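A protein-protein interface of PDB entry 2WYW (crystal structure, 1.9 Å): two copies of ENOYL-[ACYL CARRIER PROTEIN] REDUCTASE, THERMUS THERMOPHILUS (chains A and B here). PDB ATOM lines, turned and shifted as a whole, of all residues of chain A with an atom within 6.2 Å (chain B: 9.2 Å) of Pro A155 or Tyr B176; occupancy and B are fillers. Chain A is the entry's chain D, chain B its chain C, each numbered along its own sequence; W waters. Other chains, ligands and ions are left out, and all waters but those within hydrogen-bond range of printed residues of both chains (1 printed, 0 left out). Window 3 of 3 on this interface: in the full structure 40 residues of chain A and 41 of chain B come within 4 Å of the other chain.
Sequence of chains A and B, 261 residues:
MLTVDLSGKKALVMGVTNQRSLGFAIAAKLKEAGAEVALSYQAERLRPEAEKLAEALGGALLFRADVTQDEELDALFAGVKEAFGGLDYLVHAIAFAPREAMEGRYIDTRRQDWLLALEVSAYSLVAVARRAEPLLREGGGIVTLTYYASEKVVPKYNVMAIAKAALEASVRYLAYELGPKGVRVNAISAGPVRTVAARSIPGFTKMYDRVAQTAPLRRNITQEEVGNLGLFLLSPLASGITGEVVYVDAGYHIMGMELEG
Water W1 bridges OE2 of Glu B177 (2.6 Å) and OD1 of Asn A158 (3.1 Å).
The backbone NH (N) of Lys A156 lies within hydrogen-bond range of the side-chain amide oxygen (OD1) of Asn A158 (3.2 Å).
Among the printed residues, merely in contact across the chains: Pro A155 with Tyr B176 (3.4 Å), Val A153 with Arg B172 (3.5 Å), Asn A158 with Tyr B173 (3.6 Å), Val A153 with Tyr B176 (3.8 Å), Tyr A157 with Tyr B173 (3.9 Å) and Val A153 with Tyr B173 (3.9 Å).
The backbone carbonyl oxygen (O) of Val A154 lies within hydrogen-bond range of the side-chain hydroxyl (OH) of Tyr B173, at 2.7 Å.
Hydrophobic or aromatic side chains of chain A that line the printed part of chain B: Val A153, Val A154, Pro A155 and Tyr A157.
Among the printed residues, no Asp or Glu carboxylate lies within 4 Å of a Lys or Arg side-chain nitrogen of the other chain.
Pro A155 touches just one residue of chain B: Tyr B176 (3.4 Å).
Of chain A, only Val A153 (3.8 Å) and Pro A155 (3.4 Å) come within 4 Å of Tyr B176.
Val A154 touches just one residue of chain B: Tyr B173 (2.7 Å).
Printed residues of chain A within 4 Å of Tyr B173: Val A153 (3.9 Å), Val A154 (2.7 Å), Tyr A157 (3.9 Å) and Asn A158 (3.6 Å).
Of the printed residues of chain B, Tyr A157 touches Tyr B173.
Of the printed residues of chain A, Arg B172 touches Val A153 (3.5 Å).
Of the printed residues of chain B, Val A153 touches Arg B172 (3.5 Å), Tyr B173 (3.9 Å) and Tyr B176 (3.8 Å).
The nearest residue of chain A that does not touch Tyr B176 is Lys A156 (5.9 Å).
The nearest printed residue of chain B that does not touch Tyr A157 is Glu B177 (7.9 Å).
No position is printed for both chains.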
ATOM      1  N   VAL A 153      22.851 -11.358  -8.987  1.00  0.00           N
ATOM      2  CA  VAL A 153      23.898 -12.338  -8.816  1.00  0.00           C
ATOM      3  C   VAL A 153      23.715 -13.125  -7.513  1.00  0.00           C
ATOM      4  O   VAL A 153      23.739 -12.562  -6.416  1.00  0.00           O
ATOM      5  CB  VAL A 153      25.296 -11.657  -8.865  1.00  0.00           C
ATOM      6  CG1 VAL A 153      26.432 -12.645  -8.602  1.00  0.00           C
ATOM      7  CG2 VAL A 153      25.477 -10.944 -10.216  1.00  0.00           C
ATOM      8  N   VAL A 154      23.488 -14.425  -7.678  1.00  0.00           N
ATOM      9  CA  VAL A 154      23.522 -15.386  -6.597  1.00  0.00           C
ATOM     10  C   VAL A 154      24.743 -16.255  -6.865  1.00  0.00           C
ATOM     11  O   VAL A 154      24.757 -17.066  -7.770  1.00  0.00           O
ATOM     12  CB  VAL A 154      22.253 -16.237  -6.532  1.00  0.00           C
ATOM     13  CG1 VAL A 154      22.408 -17.329  -5.457  1.00  0.00           C
ATOM     14  CG2 VAL A 154      21.037 -15.344  -6.272  1.00  0.00           C
ATOM     15  N   PRO A 155      25.807 -16.046  -6.104  1.00  0.00           N
ATOM     16  CA  PRO A 155      27.007 -16.859  -6.287  1.00  0.00           C
ATOM     17  C   PRO A 155      26.708 -18.359  -6.200  1.00  0.00           C
ATOM     18  O   PRO A 155      25.768 -18.770  -5.515  1.00  0.00           O
ATOM     19  CB  PRO A 155      27.930 -16.396  -5.151  1.00  0.00           C
ATOM     20  CG  PRO A 155      27.490 -14.956  -4.879  1.00  0.00           C
ATOM     21  CD  PRO A 155      25.986 -14.984  -5.100  1.00  0.00           C
ATOM     22  N   LYS A 156      27.478 -19.137  -6.949  1.00  0.00           N
ATOM     23  CA  LYS A 156      27.306 -20.577  -7.083  1.00  0.00           C
ATOM     24  C   LYS A 156      26.097 -21.041  -7.895  1.00  0.00           C
ATOM     25  O   LYS A 156      26.062 -22.202  -8.269  1.00  0.00           O
ATOM     26  CB  LYS A 156      27.315 -21.273  -5.708  1.00  0.00           C
ATOM     27  CG  LYS A 156      28.531 -20.912  -4.854  1.00  0.00           C
ATOM     28  CD  LYS A 156      29.817 -21.168  -5.649  1.00  0.00           C
ATOM     29  CE  LYS A 156      31.070 -21.005  -4.802  1.00  0.00           C
ATOM     30  NZ  LYS A 156      32.264 -21.138  -5.687  1.00  0.00           N
ATOM     31  N   TYR A 157      25.104 -20.186  -8.160  1.00  0.00           N
ATOM     32  CA  TYR A 157      24.051 -20.542  -9.119  1.00  0.00           C
ATOM     33  C   TYR A 157      24.617 -20.437 -10.563  1.00  0.00           C
ATOM     34  O   TYR A 157      24.195 -21.152 -11.475  1.00  0.00           O
ATOM     35  CB  TYR A 157      22.816 -19.660  -8.903  1.00  0.00           C
ATOM     36  CG  TYR A 157      21.538 -20.165  -9.520  1.00  0.00           C
ATOM     37  CD1 TYR A 157      20.924 -21.324  -9.060  1.00  0.00           C
ATOM     38  CD2 TYR A 157      20.898 -19.449 -10.527  1.00  0.00           C
ATOM     39  CE1 TYR A 157      19.725 -21.781  -9.612  1.00  0.00           C
ATOM     40  CE2 TYR A 157      19.703 -19.894 -11.084  1.00  0.00           C
ATOM     41  CZ  TYR A 157      19.111 -21.048 -10.626  1.00  0.00           C
ATOM     42  OH  TYR A 157      17.901 -21.464 -11.171  1.00  0.00           O
ATOM     43  N   ASN A 158      25.564 -19.521 -10.741  1.00  0.00           N
ATOM     44  CA  ASN A 158      26.478 -19.508 -11.897  1.00  0.00           C
ATOM     45  C   ASN A 158      25.727 -19.620 -13.228  1.00  0.00           C
ATOM     46  O   ASN A 158      24.766 -18.861 -13.433  1.00  0.00           O
ATOM     47  CB  ASN A 158      27.573 -20.583 -11.705  1.00  0.00           C
ATOM     48  CG  ASN A 158      28.525 -20.258 -10.580  1.00  0.00           C
ATOM     49  OD1 ASN A 158      28.438 -19.204  -9.949  1.00  0.00           O
ATOM     50  ND2 ASN A 158      29.450 -21.173 -10.315  1.00  0.00           N
ATOM     51  N   ILE A 201      22.708 -27.200  -5.992  1.00  0.00           N
ATOM     52  CA  ILE A 201      23.253 -25.853  -5.813  1.00  0.00           C
ATOM     53  C   ILE A 201      24.086 -25.832  -4.536  1.00  0.00           C
ATOM     54  O   ILE A 201      23.535 -26.013  -3.444  1.00  0.00           O
ATOM     55  CB  ILE A 201      22.157 -24.772  -5.680  1.00  0.00           C
ATOM     56  CG1 ILE A 201      21.213 -24.794  -6.881  1.00  0.00           C
ATOM     57  CG2 ILE A 201      22.803 -23.379  -5.513  1.00  0.00           C
ATOM     58  CD1 ILE A 201      19.909 -24.059  -6.606  1.00  0.00           C
ATOM     59  N   PRO A 202      25.413 -25.605  -4.658  1.00  0.00           N
ATOM     60  CA  PRO A 202      26.219 -25.456  -3.443  1.00  0.00           C
ATOM     61  C   PRO A 202      25.640 -24.383  -2.529  1.00  0.00           C
ATOM     62  O   PRO A 202      25.296 -23.285  -2.998  1.00  0.00           O
ATOM     63  CB  PRO A 202      27.592 -25.011  -3.965  1.00  0.00           C
ATOM     64  CG  PRO A 202      27.661 -25.513  -5.360  1.00  0.00           C
ATOM     65  CD  PRO A 202      26.236 -25.482  -5.883  1.00  0.00           C
ATOM     66  N   MET A 207      21.100 -20.729   1.757  1.00  0.00           N
ATOM     67  CA  MET A 207      20.196 -19.889   0.969  1.00  0.00           C
ATOM     68  C   MET A 207      18.759 -20.049   1.481  1.00  0.00           C
ATOM     69  O   MET A 207      18.055 -19.065   1.675  1.00  0.00           O
ATOM     70  CB  MET A 207      20.199 -20.287  -0.517  1.00  0.00           C
ATOM     71  CG  MET A 207      21.521 -20.133  -1.245  1.00  0.00           C
ATOM     72  SD  MET A 207      21.398 -20.688  -2.966  1.00  0.00           S
ATOM     73  CE  MET A 207      23.097 -20.335  -3.482  1.00  0.00           C
ATOM     74  N   GLU B 133      41.541 -12.469 -17.729  1.00  0.00           N
ATOM     75  CA  GLU B 133      41.651 -12.275 -16.279  1.00  0.00           C
ATOM     76  C   GLU B 133      43.098 -12.171 -15.723  1.00  0.00           C
ATOM     77  O   GLU B 133      43.420 -11.211 -15.031  1.00  0.00           O
ATOM     78  CB  GLU B 133      40.867 -13.360 -15.522  1.00  0.00           C
ATOM     79  CG  GLU B 133      41.016 -13.210 -14.002  1.00  0.00           C
ATOM     80  CD  GLU B 133      40.286 -14.251 -13.207  1.00  0.00           C
ATOM     81  OE1 GLU B 133      40.108 -15.370 -13.686  1.00  0.00           O
ATOM     82  OE2 GLU B 133      39.913 -13.946 -12.064  1.00  0.00           O
ATOM     83  N   ALA B 169      23.212 -11.053 -18.139  1.00  0.00           N
ATOM     84  CA  ALA B 169      23.368 -11.865 -16.910  1.00  0.00           C
ATOM     85  C   ALA B 169      24.859 -12.223 -16.739  1.00  0.00           C
ATOM     86  O   ALA B 169      25.382 -12.176 -15.627  1.00  0.00           O
ATOM     87  CB  ALA B 169      22.483 -13.116 -16.971  1.00  0.00           C
ATOM     88  N   SER B 170      25.542 -12.538 -17.835  1.00  0.00           N
ATOM     89  CA  SER B 170      26.981 -12.866 -17.801  1.00  0.00           C
ATOM     90  C   SER B 170      27.785 -11.675 -17.300  1.00  0.00           C
ATOM     91  O   SER B 170      28.708 -11.826 -16.486  1.00  0.00           O
ATOM     92  CB  SER B 170      27.503 -13.280 -19.183  1.00  0.00           C
ATOM     93  OG  SER B 170      26.834 -14.434 -19.650  1.00  0.00           O
ATOM     94  N   VAL B 171      27.421 -10.478 -17.770  1.00  0.00           N
ATOM     95  CA  VAL B 171      28.067  -9.249 -17.303  1.00  0.00           C
ATOM     96  C   VAL B 171      27.936  -9.068 -15.787  1.00  0.00           C
ATOM     97  O   VAL B 171      28.867  -8.600 -15.120  1.00  0.00           O
ATOM     98  CB  VAL B 171      27.523  -7.994 -18.051  1.00  0.00           C
ATOM     99  CG1 VAL B 171      27.843  -6.700 -17.266  1.00  0.00           C
ATOM    100  CG2 VAL B 171      28.093  -7.919 -19.503  1.00  0.00           C
ATOM    101  N   ARG B 172      26.776  -9.382 -15.228  1.00  0.00           N
ATOM    102  CA  ARG B 172      26.607  -9.225 -13.794  1.00  0.00           C
ATOM    103  C   ARG B 172      27.511 -10.189 -13.024  1.00  0.00           C
ATOM    104  O   ARG B 172      28.204  -9.779 -12.102  1.00  0.00           O
ATOM    105  CB  ARG B 172      25.138  -9.388 -13.414  1.00  0.00           C
ATOM    106  CG  ARG B 172      24.300  -8.215 -13.879  1.00  0.00           C
ATOM    107  CD  ARG B 172      22.875  -8.366 -13.413  1.00  0.00           C
ATOM    108  NE  ARG B 172      22.114  -9.346 -14.164  1.00  0.00           N
ATOM    109  CZ  ARG B 172      21.439  -9.085 -15.280  1.00  0.00           C
ATOM    110  NH1 ARG B 172      21.508  -7.884 -15.834  1.00  0.00           N
ATOM    111  NH2 ARG B 172      20.716 -10.041 -15.859  1.00  0.00           N
ATOM    112  N   TYR B 173      27.554 -11.434 -13.465  1.00  0.00           N
ATOM    113  CA  TYR B 173      28.347 -12.461 -12.777  1.00  0.00           C
ATOM    114  C   TYR B 173      29.840 -12.203 -12.901  1.00  0.00           C
ATOM    115  O   TYR B 173      30.571 -12.345 -11.934  1.00  0.00           O
ATOM    116  CB  TYR B 173      27.979 -13.876 -13.268  1.00  0.00           C
ATOM    117  CG  TYR B 173      26.877 -14.501 -12.444  1.00  0.00           C
ATOM    118  CD1 TYR B 173      27.168 -15.430 -11.426  1.00  0.00           C
ATOM    119  CD2 TYR B 173      25.547 -14.132 -12.628  1.00  0.00           C
ATOM    120  CE1 TYR B 173      26.151 -15.992 -10.649  1.00  0.00           C
ATOM    121  CE2 TYR B 173      24.540 -14.668 -11.845  1.00  0.00           C
ATOM    122  CZ  TYR B 173      24.847 -15.602 -10.860  1.00  0.00           C
ATOM    123  OH  TYR B 173      23.815 -16.137 -10.108  1.00  0.00           O
ATOM    124  N   LEU B 174      30.282 -11.791 -14.088  1.00  0.00           N
ATOM    125  CA  LEU B 174      31.695 -11.491 -14.318  1.00  0.00           C
ATOM    126  C   LEU B 174      32.131 -10.253 -13.521  1.00  0.00           C
ATOM    127  O   LEU B 174      33.263 -10.223 -13.017  1.00  0.00           O
ATOM    128  CB  LEU B 174      31.979 -11.334 -15.809  1.00  0.00           C
ATOM    129  CG  LEU B 174      31.756 -12.648 -16.584  1.00  0.00           C
ATOM    130  CD1 LEU B 174      31.840 -12.454 -18.098  1.00  0.00           C
ATOM    131  CD2 LEU B 174      32.759 -13.734 -16.123  1.00  0.00           C
ATOM    132  N   ALA B 175      31.237  -9.267 -13.380  1.00  0.00           N
ATOM    133  CA  ALA B 175      31.505  -8.078 -12.576  1.00  0.00           C
ATOM    134  C   ALA B 175      31.753  -8.499 -11.119  1.00  0.00           C
ATOM    135  O   ALA B 175      32.668  -8.017 -10.453  1.00  0.00           O
ATOM    136  CB  ALA B 175      30.323  -7.087 -12.641  1.00  0.00           C
ATOM    137  N   TYR B 176      30.880  -9.358 -10.620  1.00  0.00           N
ATOM    138  CA  TYR B 176      31.026  -9.918  -9.288  1.00  0.00           C
ATOM    139  C   TYR B 176      32.388 -10.619  -9.168  1.00  0.00           C
ATOM    140  O   TYR B 176      33.126 -10.389  -8.223  1.00  0.00           O
ATOM    141  CB  TYR B 176      29.873 -10.882  -8.987  1.00  0.00           C
ATOM    142  CG  TYR B 176      30.103 -11.780  -7.792  1.00  0.00           C
ATOM    143  CD1 TYR B 176      30.297 -11.244  -6.515  1.00  0.00           C
ATOM    144  CD2 TYR B 176      30.108 -13.165  -7.931  1.00  0.00           C
ATOM    145  CE1 TYR B 176      30.523 -12.075  -5.411  1.00  0.00           C
ATOM    146  CE2 TYR B 176      30.321 -13.997  -6.843  1.00  0.00           C
ATOM    147  CZ  TYR B 176      30.543 -13.440  -5.588  1.00  0.00           C
ATOM    148  OH  TYR B 176      30.752 -14.276  -4.511  1.00  0.00           O
ATOM    149  N   GLU B 177      32.733 -11.435 -10.145  1.00  0.00           N
ATOM    150  CA  GLU B 177      33.941 -12.259 -10.020  1.00  0.00           C
ATOM    151  C   GLU B 177      35.240 -11.515 -10.291  1.00  0.00           C
ATOM    152  O   GLU B 177      36.277 -11.863  -9.714  1.00  0.00           O
ATOM    153  CB  GLU B 177      33.791 -13.527 -10.859  1.00  0.00           C
ATOM    154  CG  GLU B 177      32.645 -14.363 -10.333  1.00  0.00           C
ATOM    155  CD  GLU B 177      32.364 -15.602 -11.151  1.00  0.00           C
ATOM    156  OE1 GLU B 177      32.843 -15.684 -12.297  1.00  0.00           O
ATOM    157  OE2 GLU B 177      31.661 -16.497 -10.643  1.00  0.00           O
ATOM    158  N   LEU B 178      35.210 -10.468 -11.114  1.00  0.00           N
ATOM    159  CA  LEU B 178      36.455  -9.741 -11.422  1.00  0.00           C
ATOM    160  C   LEU B 178      36.655  -8.517 -10.529  1.00  0.00           C
ATOM    161  O   LEU B 178      37.739  -7.911 -10.509  1.00  0.00           O
ATOM    162  CB  LEU B 178      36.520  -9.377 -12.911  1.00  0.00           C
ATOM    163  CG  LEU B 178      36.615 -10.565 -13.883  1.00  0.00           C
ATOM    164  CD1 LEU B 178      36.243 -10.183 -15.315  1.00  0.00           C
ATOM    165  CD2 LEU B 178      38.037 -11.196 -13.823  1.00  0.00           C
ATOM    166  N   GLY B 179      35.621  -8.167  -9.771  1.00  0.00           N
ATOM    167  CA  GLY B 179      35.628  -6.977  -8.941  1.00  0.00           C
ATOM    168  C   GLY B 179      36.690  -6.889  -7.847  1.00  0.00           C
ATOM    169  O   GLY B 179      37.242  -5.810  -7.627  1.00  0.00           O
ATOM    170  N   PRO B 180      36.969  -8.012  -7.155  1.00  0.00           N
ATOM    171  CA  PRO B 180      38.015  -8.102  -6.109  1.00  0.00           C
ATOM    172  C   PRO B 180      39.380  -7.654  -6.610  1.00  0.00           C
ATOM    173  O   PRO B 180      40.191  -7.116  -5.864  1.00  0.00           O
ATOM    174  CB  PRO B 180      38.077  -9.609  -5.812  1.00  0.00           C
ATOM    175  CG  PRO B 180      36.719 -10.100  -6.095  1.00  0.00           C
ATOM    176  CD  PRO B 180      36.205  -9.271  -7.253  1.00  0.00           C
ATOM    177  N   LYS B 181      39.583  -7.893  -7.892  1.00  0.00           N
ATOM    178  CA  LYS B 181      40.776  -7.568  -8.631  1.00  0.00           C
ATOM    179  C   LYS B 181      40.767  -6.119  -9.146  1.00  0.00           C
ATOM    180  O   LYS B 181      41.698  -5.699  -9.806  1.00  0.00           O
ATOM    181  CB  LYS B 181      40.776  -8.548  -9.796  1.00  0.00           C
ATOM    182  CG  LYS B 181      41.940  -8.668 -10.651  1.00  0.00           C
ATOM    183  CD  LYS B 181      41.629  -9.785 -11.667  1.00  0.00           C
ATOM    184  CE  LYS B 181      42.872 -10.328 -12.307  1.00  0.00           C
ATOM    185  NZ  LYS B 181      43.708 -11.114 -11.359  1.00  0.00           N
ATOM    186  N   GLY B 182      39.711  -5.361  -8.860  1.00  0.00           N
ATOM    187  CA  GLY B 182      39.606  -3.977  -9.325  1.00  0.00           C
ATOM    188  C   GLY B 182      39.378  -3.886 -10.821  1.00  0.00           C
ATOM    189  O   GLY B 182      39.752  -2.900 -11.448  1.00  0.00           O
ATOM    190  N   VAL B 183      38.765  -4.920 -11.388  1.00  0.00           N
ATOM    191  CA  VAL B 183      38.385  -4.930 -12.804  1.00  0.00           C
ATOM    192  C   VAL B 183      36.862  -4.800 -12.901  1.00  0.00           C
ATOM    193  O   VAL B 183      36.120  -5.442 -12.163  1.00  0.00           O
ATOM    194  CB  VAL B 183      38.842  -6.199 -13.466  1.00  0.00           C
ATOM    195  CG1 VAL B 183      38.266  -6.322 -14.931  1.00  0.00           C
ATOM    196  CG2 VAL B 183      40.367  -6.270 -13.410  1.00  0.00           C
ATOM    197  N   ARG B 184      36.404  -3.920 -13.779  1.00  0.00           N
ATOM    198  CA  ARG B 184      34.971  -3.674 -13.912  1.00  0.00           C
ATOM    199  C   ARG B 184      34.490  -4.346 -15.191  1.00  0.00           C
ATOM    200  O   ARG B 184      35.269  -4.559 -16.119  1.00  0.00           O
ATOM    201  CB  ARG B 184      34.694  -2.184 -13.890  1.00  0.00           C
ATOM    202  CG  ARG B 184      35.158  -1.571 -12.587  1.00  0.00           C
ATOM    203  CD  ARG B 184      34.902  -0.104 -12.483  1.00  0.00           C
ATOM    204  NE  ARG B 184      35.765   0.696 -13.342  1.00  0.00           N
ATOM    205  CZ  ARG B 184      35.398   1.282 -14.485  1.00  0.00           C
ATOM    206  NH1 ARG B 184      34.158   1.142 -14.985  1.00  0.00           N
ATOM    207  NH2 ARG B 184      36.292   2.003 -15.149  1.00  0.00           N
ATOM    208  N   VAL B 185      33.226  -4.734 -15.210  1.00  0.00           N
ATOM    209  CA  VAL B 185      32.605  -5.312 -16.388  1.00  0.00           C
ATOM    210  C   VAL B 185      31.248  -4.594 -16.576  1.00  0.00           C
ATOM    211  O   VAL B 185      30.467  -4.516 -15.639  1.00  0.00           O
ATOM    212  CB  VAL B 185      32.399  -6.841 -16.234  1.00  0.00           C
ATOM    213  CG1 VAL B 185      31.747  -7.434 -17.501  1.00  0.00           C
ATOM    214  CG2 VAL B 185      33.742  -7.594 -15.876  1.00  0.00           C
ATOM    215  N   ASN B 186      30.982  -4.096 -17.782  1.00  0.00           N
ATOM    216  CA  ASN B 186      29.734  -3.419 -18.075  1.00  0.00           C
ATOM    217  C   ASN B 186      29.267  -3.744 -19.492  1.00  0.00           C
ATOM    218  O   ASN B 186      30.074  -4.215 -20.306  1.00  0.00           O
ATOM    219  CB  ASN B 186      29.882  -1.911 -17.932  1.00  0.00           C
ATOM    220  CG  ASN B 186      30.213  -1.479 -16.515  1.00  0.00           C
ATOM    221  OD1 ASN B 186      29.337  -1.425 -15.651  1.00  0.00           O
ATOM    222  ND2 ASN B 186      31.489  -1.172 -16.269  1.00  0.00           N
ATOM    223  N   THR B 242      30.149  -0.700 -12.235  1.00  0.00           N
ATOM    224  CA  THR B 242      30.362  -2.058 -12.686  1.00  0.00           C
ATOM    225  C   THR B 242      29.088  -2.875 -12.621  1.00  0.00           C
ATOM    226  O   THR B 242      28.194  -2.589 -11.829  1.00  0.00           O
ATOM    227  CB  THR B 242      31.547  -2.769 -11.914  1.00  0.00           C
ATOM    228  OG1 THR B 242      31.964  -3.928 -12.647  1.00  0.00           O
ATOM    229  CG2 THR B 242      31.179  -3.141 -10.510  1.00  0.00           C
ATOM    230  N   GLY B 243      29.026  -3.894 -13.484  1.00  0.00           N
ATOM    231  CA  GLY B 243      27.850  -4.735 -13.632  1.00  0.00           C
ATOM    232  C   GLY B 243      26.639  -4.070 -14.248  1.00  0.00           C
ATOM    233  O   GLY B 243      25.552  -4.625 -14.196  1.00  0.00           O
ATOM    234  N   GLU B 244      26.835  -2.924 -14.899  1.00  0.00           N
ATOM    235  CA  GLU B 244      25.734  -2.118 -15.422  1.00  0.00           C
ATOM    236  C   GLU B 244      25.486  -2.361 -16.888  1.00  0.00           C
ATOM    237  O   GLU B 244      26.410  -2.692 -17.632  1.00  0.00           O
ATOM    238  CB  GLU B 244      26.062  -0.633 -15.260  1.00  0.00           C
ATOM    239  CG  GLU B 244      26.384  -0.308 -13.824  1.00  0.00           C
ATOM    240  CD  GLU B 244      25.281  -0.795 -12.913  1.00  0.00           C
ATOM    241  OE1 GLU B 244      24.105  -0.404 -13.233  1.00  0.00           O
ATOM    242  OE2 GLU B 244      25.591  -1.555 -11.927  1.00  0.00           O
HETATM  243  O   HOH W   1      29.722 -16.655  -8.873  1.00  0.00           O
